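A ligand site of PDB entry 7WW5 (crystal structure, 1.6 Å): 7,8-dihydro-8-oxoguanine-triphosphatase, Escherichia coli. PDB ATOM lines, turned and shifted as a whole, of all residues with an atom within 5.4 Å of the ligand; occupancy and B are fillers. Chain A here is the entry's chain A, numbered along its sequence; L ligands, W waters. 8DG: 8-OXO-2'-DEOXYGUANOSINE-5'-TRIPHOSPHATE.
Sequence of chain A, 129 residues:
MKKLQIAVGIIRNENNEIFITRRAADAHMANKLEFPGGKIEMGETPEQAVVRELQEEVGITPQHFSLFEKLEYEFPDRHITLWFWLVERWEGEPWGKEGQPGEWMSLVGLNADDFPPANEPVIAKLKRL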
ATOM      1  N   ILE A   6     -16.587  27.056 -13.373  1.00  0.00           N
ATOM      2  CA  ILE A   6     -17.776  26.247 -13.582  1.00  0.00           C
ATOM      3  C   ILE A   6     -19.011  27.117 -13.408  1.00  0.00           C
ATOM      4  O   ILE A   6     -19.147  27.809 -12.390  1.00  0.00           O
ATOM      5  CB  ILE A   6     -17.808  25.045 -12.617  1.00  0.00           C
ATOM      6  CG1 ILE A   6     -16.532  24.190 -12.694  1.00  0.00           C
ATOM      7  CG2 ILE A   6     -19.073  24.188 -12.858  1.00  0.00           C
ATOM      8  CD1 ILE A   6     -16.226  23.596 -14.069  1.00  0.00           C
ATOM      9  N   VAL A   8     -23.176  26.937 -13.130  1.00  0.00           N
ATOM     10  CA  VAL A   8     -24.283  26.020 -12.893  1.00  0.00           C
ATOM     11  C   VAL A   8     -25.570  26.814 -12.713  1.00  0.00           C
ATOM     12  O   VAL A   8     -25.563  28.010 -12.394  1.00  0.00           O
ATOM     13  CB  VAL A   8     -24.024  25.096 -11.672  1.00  0.00           C
ATOM     14  CG1 VAL A   8     -22.678  24.428 -11.787  1.00  0.00           C
ATOM     15  CG2 VAL A   8     -24.156  25.858 -10.372  1.00  0.00           C
ATOM     16  N   ARG A  23     -24.873  13.054 -11.397  1.00  0.00           N
ATOM     17  CA  ARG A  23     -23.677  12.863 -12.183  1.00  0.00           C
ATOM     18  C   ARG A  23     -23.372  11.382 -12.387  1.00  0.00           C
ATOM     19  O   ARG A  23     -23.700  10.533 -11.545  1.00  0.00           O
ATOM     20  CB  ARG A  23     -22.490  13.554 -11.513  1.00  0.00           C
ATOM     21  CG  ARG A  23     -22.749  15.026 -11.260  1.00  0.00           C
ATOM     22  CD  ARG A  23     -21.623  15.735 -10.534  1.00  0.00           C
ATOM     23  NE  ARG A  23     -20.333  15.659 -11.215  1.00  0.00           N
ATOM     24  CZ  ARG A  23     -19.954  16.413 -12.242  1.00  0.00           C
ATOM     25  NH1 ARG A  23     -20.769  17.334 -12.744  1.00  0.00           N
ATOM     26  NH2 ARG A  23     -18.750  16.237 -12.763  1.00  0.00           N
ATOM     27  N   HIS A  28     -16.072  13.043 -12.235  1.00  0.00           N
ATOM     28  CA  HIS A  28     -15.682  13.672 -10.987  1.00  0.00           C
ATOM     29  C   HIS A  28     -16.946  13.947 -10.180  1.00  0.00           C
ATOM     30  O   HIS A  28     -17.994  14.262 -10.748  1.00  0.00           O
ATOM     31  CB  HIS A  28     -14.921  14.968 -11.245  1.00  0.00           C
ATOM     32  CG  HIS A  28     -14.377  15.597 -10.008  1.00  0.00           C
ATOM     33  ND1 HIS A  28     -14.911  16.736  -9.454  1.00  0.00           N
ATOM     34  CD2 HIS A  28     -13.347  15.230  -9.199  1.00  0.00           C
ATOM     35  CE1 HIS A  28     -14.243  17.048  -8.353  1.00  0.00           C
ATOM     36  NE2 HIS A  28     -13.281  16.147  -8.180  1.00  0.00           N
ATOM     37  N   MET A  29     -16.857  13.832  -8.853  1.00  0.00           N
ATOM     38  CA  MET A  29     -18.044  13.868  -7.995  1.00  0.00           C
ATOM     39  C   MET A  29     -19.080  12.861  -8.480  1.00  0.00           C
ATOM     40  O   MET A  29     -20.254  13.172  -8.671  1.00  0.00           O
ATOM     41  CB  MET A  29     -18.630  15.279  -7.898  1.00  0.00           C
ATOM     42  CG  MET A  29     -17.767  16.213  -7.029  1.00  0.00           C
ATOM     43  SD  MET A  29     -17.717  15.649  -5.322  1.00  0.00           S
ATOM     44  CE  MET A  29     -16.143  14.800  -5.248  1.00  0.00           C
ATOM     45  N   LEU A  33     -25.816  14.285  -6.678  1.00  0.00           N
ATOM     46  CA  LEU A  33     -26.775  15.262  -7.156  1.00  0.00           C
ATOM     47  C   LEU A  33     -26.072  16.568  -7.482  1.00  0.00           C
ATOM     48  O   LEU A  33     -25.021  16.899  -6.919  1.00  0.00           O
ATOM     49  CB  LEU A  33     -27.886  15.499  -6.131  1.00  0.00           C
ATOM     50  CG  LEU A  33     -28.781  14.283  -5.877  1.00  0.00           C
ATOM     51  CD1 LEU A  33     -29.927  14.636  -4.956  1.00  0.00           C
ATOM     52  CD2 LEU A  33     -29.293  13.749  -7.208  1.00  0.00           C
ATOM     53  N   GLU A  34     -26.663  17.331  -8.398  1.00  0.00           N
ATOM     54  CA  GLU A  34     -25.976  18.528  -8.868  1.00  0.00           C
ATOM     55  C   GLU A  34     -26.980  19.487  -9.481  1.00  0.00           C
ATOM     56  O   GLU A  34     -28.080  19.093  -9.892  1.00  0.00           O
ATOM     57  CB  GLU A  34     -24.915  18.177  -9.921  1.00  0.00           C
ATOM     58  CG  GLU A  34     -25.525  17.480 -11.120  1.00  0.00           C
ATOM     59  CD  GLU A  34     -24.668  17.480 -12.367  1.00  0.00           C
ATOM     60  OE1 GLU A  34     -23.504  17.933 -12.317  1.00  0.00           O
ATOM     61  OE2 GLU A  34     -25.176  16.972 -13.391  1.00  0.00           O
ATOM     62  N   PHE A  35     -26.599  20.749  -9.530  1.00  0.00           N
ATOM     63  CA  PHE A  35     -27.234  21.699 -10.441  1.00  0.00           C
ATOM     64  C   PHE A  35     -26.643  21.516 -11.834  1.00  0.00           C
ATOM     65  O   PHE A  35     -25.423  21.379 -11.950  1.00  0.00           O
ATOM     66  CB  PHE A  35     -27.027  23.146  -9.939  1.00  0.00           C
ATOM     67  CG  PHE A  35     -27.429  23.367  -8.492  1.00  0.00           C
ATOM     68  CD1 PHE A  35     -28.736  23.195  -8.085  1.00  0.00           C
ATOM     69  CD2 PHE A  35     -26.495  23.808  -7.557  1.00  0.00           C
ATOM     70  CE1 PHE A  35     -29.129  23.403  -6.766  1.00  0.00           C
ATOM     71  CE2 PHE A  35     -26.865  24.021  -6.232  1.00  0.00           C
ATOM     72  CZ  PHE A  35     -28.188  23.810  -5.827  1.00  0.00           C
ATOM     73  N   PRO A  36     -27.446  21.466 -12.892  1.00  0.00           N
ATOM     74  CA  PRO A  36     -26.847  21.333 -14.228  1.00  0.00           C
ATOM     75  C   PRO A  36     -25.894  22.488 -14.499  1.00  0.00           C
ATOM     76  O   PRO A  36     -26.154  23.627 -14.108  1.00  0.00           O
ATOM     77  CB  PRO A  36     -28.069  21.368 -15.167  1.00  0.00           C
ATOM     78  CG  PRO A  36     -29.180  20.837 -14.319  1.00  0.00           C
ATOM     79  CD  PRO A  36     -28.915  21.421 -12.939  1.00  0.00           C
ATOM     80  N   GLY A  37     -24.790  22.169 -15.162  1.00  0.00           N
ATOM     81  CA  GLY A  37     -23.802  23.178 -15.474  1.00  0.00           C
ATOM     82  C   GLY A  37     -22.522  22.555 -15.989  1.00  0.00           C
ATOM     83  O   GLY A  37     -22.473  21.364 -16.316  1.00  0.00           O
ATOM     84  N   GLY A  38     -21.488  23.379 -16.093  1.00  0.00           N
ATOM     85  CA  GLY A  38     -20.216  22.862 -16.552  1.00  0.00           C
ATOM     86  C   GLY A  38     -19.217  23.961 -16.823  1.00  0.00           C
ATOM     87  O   GLY A  38     -19.378  25.113 -16.391  1.00  0.00           O
ATOM     88  N   LYS A  39     -18.168  23.578 -17.532  1.00  0.00           N
ATOM     89  CA  LYS A  39     -16.992  24.419 -17.681  1.00  0.00           C
ATOM     90  C   LYS A  39     -17.279  25.645 -18.548  1.00  0.00           C
ATOM     91  O   LYS A  39     -17.855  25.532 -19.630  1.00  0.00           O
ATOM     92  CB  LYS A  39     -15.860  23.606 -18.296  1.00  0.00           C
ATOM     93  CG  LYS A  39     -15.385  22.510 -17.352  1.00  0.00           C
ATOM     94  CD  LYS A  39     -14.662  21.362 -18.053  1.00  0.00           C
ATOM     95  CE  LYS A  39     -14.140  20.381 -17.008  1.00  0.00           C
ATOM     96  NZ  LYS A  39     -14.054  18.983 -17.502  1.00  0.00           N
ATOM     97  N   GLU A  53     -24.702  25.755 -21.163  1.00  0.00           N
ATOM     98  CA  GLU A  53     -24.710  24.498 -20.401  1.00  0.00           C
ATOM     99  C   GLU A  53     -26.125  23.989 -20.147  1.00  0.00           C
ATOM    100  O   GLU A  53     -26.377  22.784 -20.237  1.00  0.00           O
ATOM    101  CB  GLU A  53     -23.969  24.695 -19.090  1.00  0.00           C
ATOM    102  CG  GLU A  53     -22.452  24.818 -19.270  1.00  0.00           C
ATOM    103  CD  GLU A  53     -21.812  23.495 -19.616  1.00  0.00           C
ATOM    104  OE1 GLU A  53     -22.442  22.429 -19.338  1.00  0.00           O
ATOM    105  OE2 GLU A  53     -20.701  23.491 -20.180  1.00  0.00           O
ATOM    106  N   GLU A  57     -27.453  20.478 -21.460  1.00  0.00           N
ATOM    107  CA  GLU A  57     -27.672  19.404 -20.502  1.00  0.00           C
ATOM    108  C   GLU A  57     -29.141  19.086 -20.297  1.00  0.00           C
ATOM    109  O   GLU A  57     -29.502  17.926 -20.074  1.00  0.00           O
ATOM    110  CB  GLU A  57     -27.009  19.748 -19.170  1.00  0.00           C
ATOM    111  CG  GLU A  57     -25.496  19.640 -19.241  1.00  0.00           C
ATOM    112  CD  GLU A  57     -24.860  19.387 -17.906  1.00  0.00           C
ATOM    113  OE1 GLU A  57     -25.518  19.650 -16.873  1.00  0.00           O
ATOM    114  OE2 GLU A  57     -23.714  18.902 -17.888  1.00  0.00           O
ATOM    115  N   PHE A  75     -10.934  20.747  -4.156  1.00  0.00           N
ATOM    116  CA  PHE A  75     -11.070  19.283  -4.125  1.00  0.00           C
ATOM    117  C   PHE A  75      -9.707  18.654  -3.930  1.00  0.00           C
ATOM    118  O   PHE A  75      -8.668  19.316  -4.058  1.00  0.00           O
ATOM    119  CB  PHE A  75     -11.687  18.784  -5.434  1.00  0.00           C
ATOM    120  CG  PHE A  75     -13.142  19.068  -5.580  1.00  0.00           C
ATOM    121  CD1 PHE A  75     -14.096  18.240  -5.000  1.00  0.00           C
ATOM    122  CD2 PHE A  75     -13.571  20.157  -6.321  1.00  0.00           C
ATOM    123  CE1 PHE A  75     -15.444  18.497  -5.153  1.00  0.00           C
ATOM    124  CE2 PHE A  75     -14.913  20.421  -6.473  1.00  0.00           C
ATOM    125  CZ  PHE A  75     -15.856  19.583  -5.890  1.00  0.00           C
ATOM    126  N   ARG A  78      -8.216  19.015  -7.612  1.00  0.00           N
ATOM    127  CA  ARG A  78      -8.519  20.136  -8.491  1.00  0.00           C
ATOM    128  C   ARG A  78      -9.136  21.269  -7.695  1.00  0.00           C
ATOM    129  O   ARG A  78      -9.739  21.060  -6.639  1.00  0.00           O
ATOM    130  CB  ARG A  78      -9.455  19.719  -9.627  1.00  0.00           C
ATOM    131  CG  ARG A  78     -10.835  19.294  -9.178  1.00  0.00           C
ATOM    132  CD  ARG A  78     -11.493  18.518 -10.304  1.00  0.00           C
ATOM    133  NE  ARG A  78     -10.772  17.262 -10.516  1.00  0.00           N
ATOM    134  CZ  ARG A  78     -11.067  16.390 -11.474  1.00  0.00           C
ATOM    135  NH1 ARG A  78     -12.045  16.651 -12.320  1.00  0.00           N
ATOM    136  NH2 ARG A  78     -10.368  15.260 -11.589  1.00  0.00           N
ATOM    137  N   ILE A  80     -11.761  24.506  -8.197  1.00  0.00           N
ATOM    138  CA  ILE A  80     -12.737  25.086  -9.108  1.00  0.00           C
ATOM    139  C   ILE A  80     -13.339  26.342  -8.492  1.00  0.00           C
ATOM    140  O   ILE A  80     -13.349  26.538  -7.276  1.00  0.00           O
ATOM    141  CB  ILE A  80     -13.854  24.097  -9.506  1.00  0.00           C
ATOM    142  CG1 ILE A  80     -14.815  23.868  -8.359  1.00  0.00           C
ATOM    143  CG2 ILE A  80     -13.262  22.784  -9.981  1.00  0.00           C
ATOM    144  CD1 ILE A  80     -16.030  23.065  -8.780  1.00  0.00           C
ATOM    145  N   LEU A  82     -17.002  28.138  -8.644  1.00  0.00           N
ATOM    146  CA  LEU A  82     -18.374  27.787  -8.990  1.00  0.00           C
ATOM    147  C   LEU A  82     -19.226  29.047  -9.070  1.00  0.00           C
ATOM    148  O   LEU A  82     -19.272  29.832  -8.123  1.00  0.00           O
ATOM    149  CB  LEU A  82     -18.965  26.817  -7.968  1.00  0.00           C
ATOM    150  CG  LEU A  82     -18.623  25.347  -8.192  1.00  0.00           C
ATOM    151  CD1 LEU A  82     -18.698  24.611  -6.881  1.00  0.00           C
ATOM    152  CD2 LEU A  82     -19.578  24.722  -9.201  1.00  0.00           C
ATOM    153  N   PHE A  84     -22.923  30.076  -9.233  1.00  0.00           N
ATOM    154  CA  PHE A  84     -24.271  29.541  -9.018  1.00  0.00           C
ATOM    155  C   PHE A  84     -25.284  30.576  -9.470  1.00  0.00           C
ATOM    156  O   PHE A  84     -25.459  31.605  -8.800  1.00  0.00           O
ATOM    157  CB  PHE A  84     -24.507  29.205  -7.549  1.00  0.00           C
ATOM    158  CG  PHE A  84     -23.678  28.061  -6.999  1.00  0.00           C
ATOM    159  CD1 PHE A  84     -22.443  28.294  -6.425  1.00  0.00           C
ATOM    160  CD2 PHE A  84     -24.174  26.767  -7.030  1.00  0.00           C
ATOM    161  CE1 PHE A  84     -21.700  27.231  -5.895  1.00  0.00           C
ATOM    162  CE2 PHE A  84     -23.431  25.704  -6.500  1.00  0.00           C
ATOM    163  CZ  PHE A  84     -22.193  25.936  -5.940  1.00  0.00           C
ATOM    164  N   PHE A 115     -24.940  16.163  -2.519  1.00  0.00           N
ATOM    165  CA  PHE A 115     -24.326  17.065  -3.501  1.00  0.00           C
ATOM    166  C   PHE A 115     -22.825  17.141  -3.249  1.00  0.00           C
ATOM    167  O   PHE A 115     -22.336  16.713  -2.184  1.00  0.00           O
ATOM    168  CB  PHE A 115     -24.942  18.476  -3.404  1.00  0.00           C
ATOM    169  CG  PHE A 115     -26.374  18.581  -3.898  1.00  0.00           C
ATOM    170  CD1 PHE A 115     -27.429  18.110  -3.134  1.00  0.00           C
ATOM    171  CD2 PHE A 115     -26.664  19.183  -5.128  1.00  0.00           C
ATOM    172  CE1 PHE A 115     -28.745  18.225  -3.584  1.00  0.00           C
ATOM    173  CE2 PHE A 115     -27.960  19.305  -5.558  1.00  0.00           C
ATOM    174  CZ  PHE A 115     -29.012  18.817  -4.792  1.00  0.00           C
ATOM    175  N   PRO A 116     -22.039  17.629  -4.210  1.00  0.00           N
ATOM    176  CA  PRO A 116     -20.642  17.927  -3.913  1.00  0.00           C
ATOM    177  C   PRO A 116     -20.539  18.880  -2.747  1.00  0.00           C
ATOM    178  O   PRO A 116     -21.428  19.734  -2.546  1.00  0.00           O
ATOM    179  CB  PRO A 116     -20.131  18.556  -5.219  1.00  0.00           C
ATOM    180  CG  PRO A 116     -21.085  18.061  -6.281  1.00  0.00           C
ATOM    181  CD  PRO A 116     -22.395  18.005  -5.589  1.00  0.00           C
ATOM    182  N   ALA A 118     -18.911  21.481  -2.115  1.00  0.00           N
ATOM    183  CA  ALA A 118     -18.893  22.911  -2.439  1.00  0.00           C
ATOM    184  C   ALA A 118     -20.290  23.518  -2.407  1.00  0.00           C
ATOM    185  O   ALA A 118     -20.431  24.710  -2.164  1.00  0.00           O
ATOM    186  CB  ALA A 118     -18.264  23.123  -3.811  1.00  0.00           C
ATOM    187  N   ASN A 119     -21.328  22.704  -2.664  1.00  0.00           N
ATOM    188  CA  ASN A 119     -22.689  23.228  -2.735  1.00  0.00           C
ATOM    189  C   ASN A 119     -23.303  23.504  -1.369  1.00  0.00           C
ATOM    190  O   ASN A 119     -24.398  24.092  -1.307  1.00  0.00           O
ATOM    191  CB  ASN A 119     -23.577  22.231  -3.497  1.00  0.00           C
ATOM    192  CG  ASN A 119     -23.191  22.069  -4.967  1.00  0.00           C
ATOM    193  OD1 ASN A 119     -22.034  22.155  -5.349  1.00  0.00           O
ATOM    194  ND2 ASN A 119     -24.194  21.809  -5.808  1.00  0.00           N
HETATM  195  PG  8DG L   1     -17.216  18.208 -20.035  1.00  0.00           P
HETATM  196  O1G 8DG L   1     -15.715  18.171 -20.231  1.00  0.00           O
HETATM  197  O2G 8DG L   1     -17.910  19.310 -20.811  1.00  0.00           O
HETATM  198  O3G 8DG L   1     -17.884  16.857 -20.100  1.00  0.00           O
HETATM  199  O3B 8DG L   1     -17.390  18.629 -18.489  1.00  0.00           O
HETATM  200  PB  8DG L   1     -18.529  19.637 -17.962  1.00  0.00           P
HETATM  201  O1B 8DG L   1     -18.384  20.982 -18.613  1.00  0.00           O
HETATM  202  O2B 8DG L   1     -19.872  18.917 -17.961  1.00  0.00           O
HETATM  203  O3A 8DG L   1     -18.049  19.871 -16.451  1.00  0.00           O
HETATM  204  PA  8DG L   1     -18.549  19.045 -15.166  1.00  0.00           P
HETATM  205  O1A 8DG L   1     -20.006  19.310 -14.871  1.00  0.00           O
HETATM  206  O2A 8DG L   1     -18.039  17.626 -15.297  1.00  0.00           O
HETATM  207  O5' 8DG L   1     -17.582  19.774 -14.109  1.00  0.00           O
HETATM  208  C5' 8DG L   1     -18.124  20.429 -12.969  1.00  0.00           C
HETATM  209  C4' 8DG L   1     -17.132  20.444 -11.822  1.00  0.00           C
HETATM  210  O4' 8DG L   1     -17.732  21.226 -10.808  1.00  0.00           O
HETATM  211  C3' 8DG L   1     -16.949  19.048 -11.249  1.00  0.00           C
HETATM  212  O3' 8DG L   1     -15.653  19.035 -10.658  1.00  0.00           O
HETATM  213  C2' 8DG L   1     -18.006  18.971 -10.167  1.00  0.00           C
HETATM  214  C1' 8DG L   1     -18.036  20.415  -9.684  1.00  0.00           C
HETATM  215  N9  8DG L   1     -19.365  20.752  -9.140  1.00  0.00           N
HETATM  216  C8  8DG L   1     -19.647  21.019  -7.869  1.00  0.00           C
HETATM  217  N7  8DG L   1     -20.933  21.287  -7.625  1.00  0.00           N
HETATM  218  C5  8DG L   1     -21.493  21.200  -8.866  1.00  0.00           C
HETATM  219  C6  8DG L   1     -22.875  21.356  -9.365  1.00  0.00           C
HETATM  220  O6  8DG L   1     -23.828  21.642  -8.587  1.00  0.00           O
HETATM  221  N1  8DG L   1     -23.072  21.201 -10.682  1.00  0.00           N
HETATM  222  C2  8DG L   1     -22.068  20.881 -11.532  1.00  0.00           C
HETATM  223  N2  8DG L   1     -22.299  20.731 -12.858  1.00  0.00           N
HETATM  224  N3  8DG L   1     -20.795  20.713 -11.105  1.00  0.00           N
HETATM  225  C4  8DG L   1     -20.510  20.872  -9.794  1.00  0.00           C
HETATM  226  O8  8DG L   1     -18.747  20.993  -6.957  1.00  0.00           O
HETATM  227  O   HOH W   1     -15.390  17.295 -14.775  1.00  0.00           O
HETATM  228  O   HOH W   2     -19.262  15.968 -16.610  1.00  0.00           O
HETATM  229  O   HOH W   3     -21.377  20.118 -19.836  1.00  0.00           O
HETATM  230  O   HOH W   4     -23.728  18.803 -14.998  1.00  0.00           O
HETATM  231  O   HOH W   5     -13.834  18.748 -12.805  1.00  0.00           O
HETATM  232  O   HOH W   6     -22.003  16.829 -16.663  1.00  0.00           O
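Residues that only touch the ligand: Ile 6 (3.7 Å), Val 8 (3.4 Å), Gly 37 (3.5 Å), Gly 38 (3.3 Å), Glu 53 (3.8 Å), Glu 57 (3.8 Å), Phe 75 (3.4 Å), Ile 80 (3.2 Å), Leu 82 (3.6 Å), Pro 116 (3.3 Å) and Ala 118 (3.8 Å).
17 residues have an atom within 4 Å of the ligand: Ile 6, Val 8, Arg 23, His 28, Glu 34, Phe 35, Gly 37, Gly 38, Lys 39, Glu 53, Glu 57, Phe 75, Ile 80, Leu 82, Pro 116, Ala 118 and Asn 119.
The nearest printed residue that does not touch the ligand is Met 29 (4.2 Å).
The backbone carbonyl oxygen (O) of Phe 35 lies within hydrogen-bond range of a nitrogen (N1) of the ligand (2.7 Å).
The backbone NH (N) of Phe 35 sits at hydrogen-bond distance from an oxygen (O6) of the ligand, 3.1 Å away.
The side-chain amide oxygen (OD1) of Asn 119 sits at hydrogen-bond distance from a nitrogen (N7) of the ligand (2.7 Å).
The side-chain amino group (NZ) of Lys 39 is in salt-bridge range of an oxygen (O1G) of the ligand, at 3.3 Å.
An oxygen (O2A) of the ligand is in salt-bridge range of the guanidinium group (NH2) of Arg 23.
A ring nitrogen (ND1) of His 28 lies within hydrogen-bond range of an oxygen (O3') of the ligand, 2.7 Å away.
OE1 of Glu 34 is in hydrogen-bond range of N2 of the ligand.
The backbone NH of Lys 39 is in hydrogen-bond range of an oxygen (O1B) of the ligand.
The guanidinium group (NH1) of Arg 23 is in salt-bridge range of the side-chain carboxylate (OE1) of Glu 34, at 2.8 Å.
The guanidinium group (NE) of Arg 23 lies within hydrogen-bond range of the backbone carbonyl oxygen (O) of His 28 (2.8 Å).
The side-chain carboxylate of Glu 57 sits at hydrogen-bond distance from the backbone NH of Gly 37.
Water W3 lies within hydrogen-bond range of OE1 of Glu 53 (2.6 Å), O2B of the ligand (2.7 Å) and OE2 of Glu 57 (3.3 Å).
Water W1 bridges an oxygen (O2A) of the ligand and the side-chain amino group (NZ) of Lys 39.
Water W5 lies within hydrogen-bond range of the guanidinium group of Arg 78 and an oxygen (O3') of the ligand.
Water W6 lies within hydrogen-bond range of OE2 of Glu 57 and O2B of the ligand.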
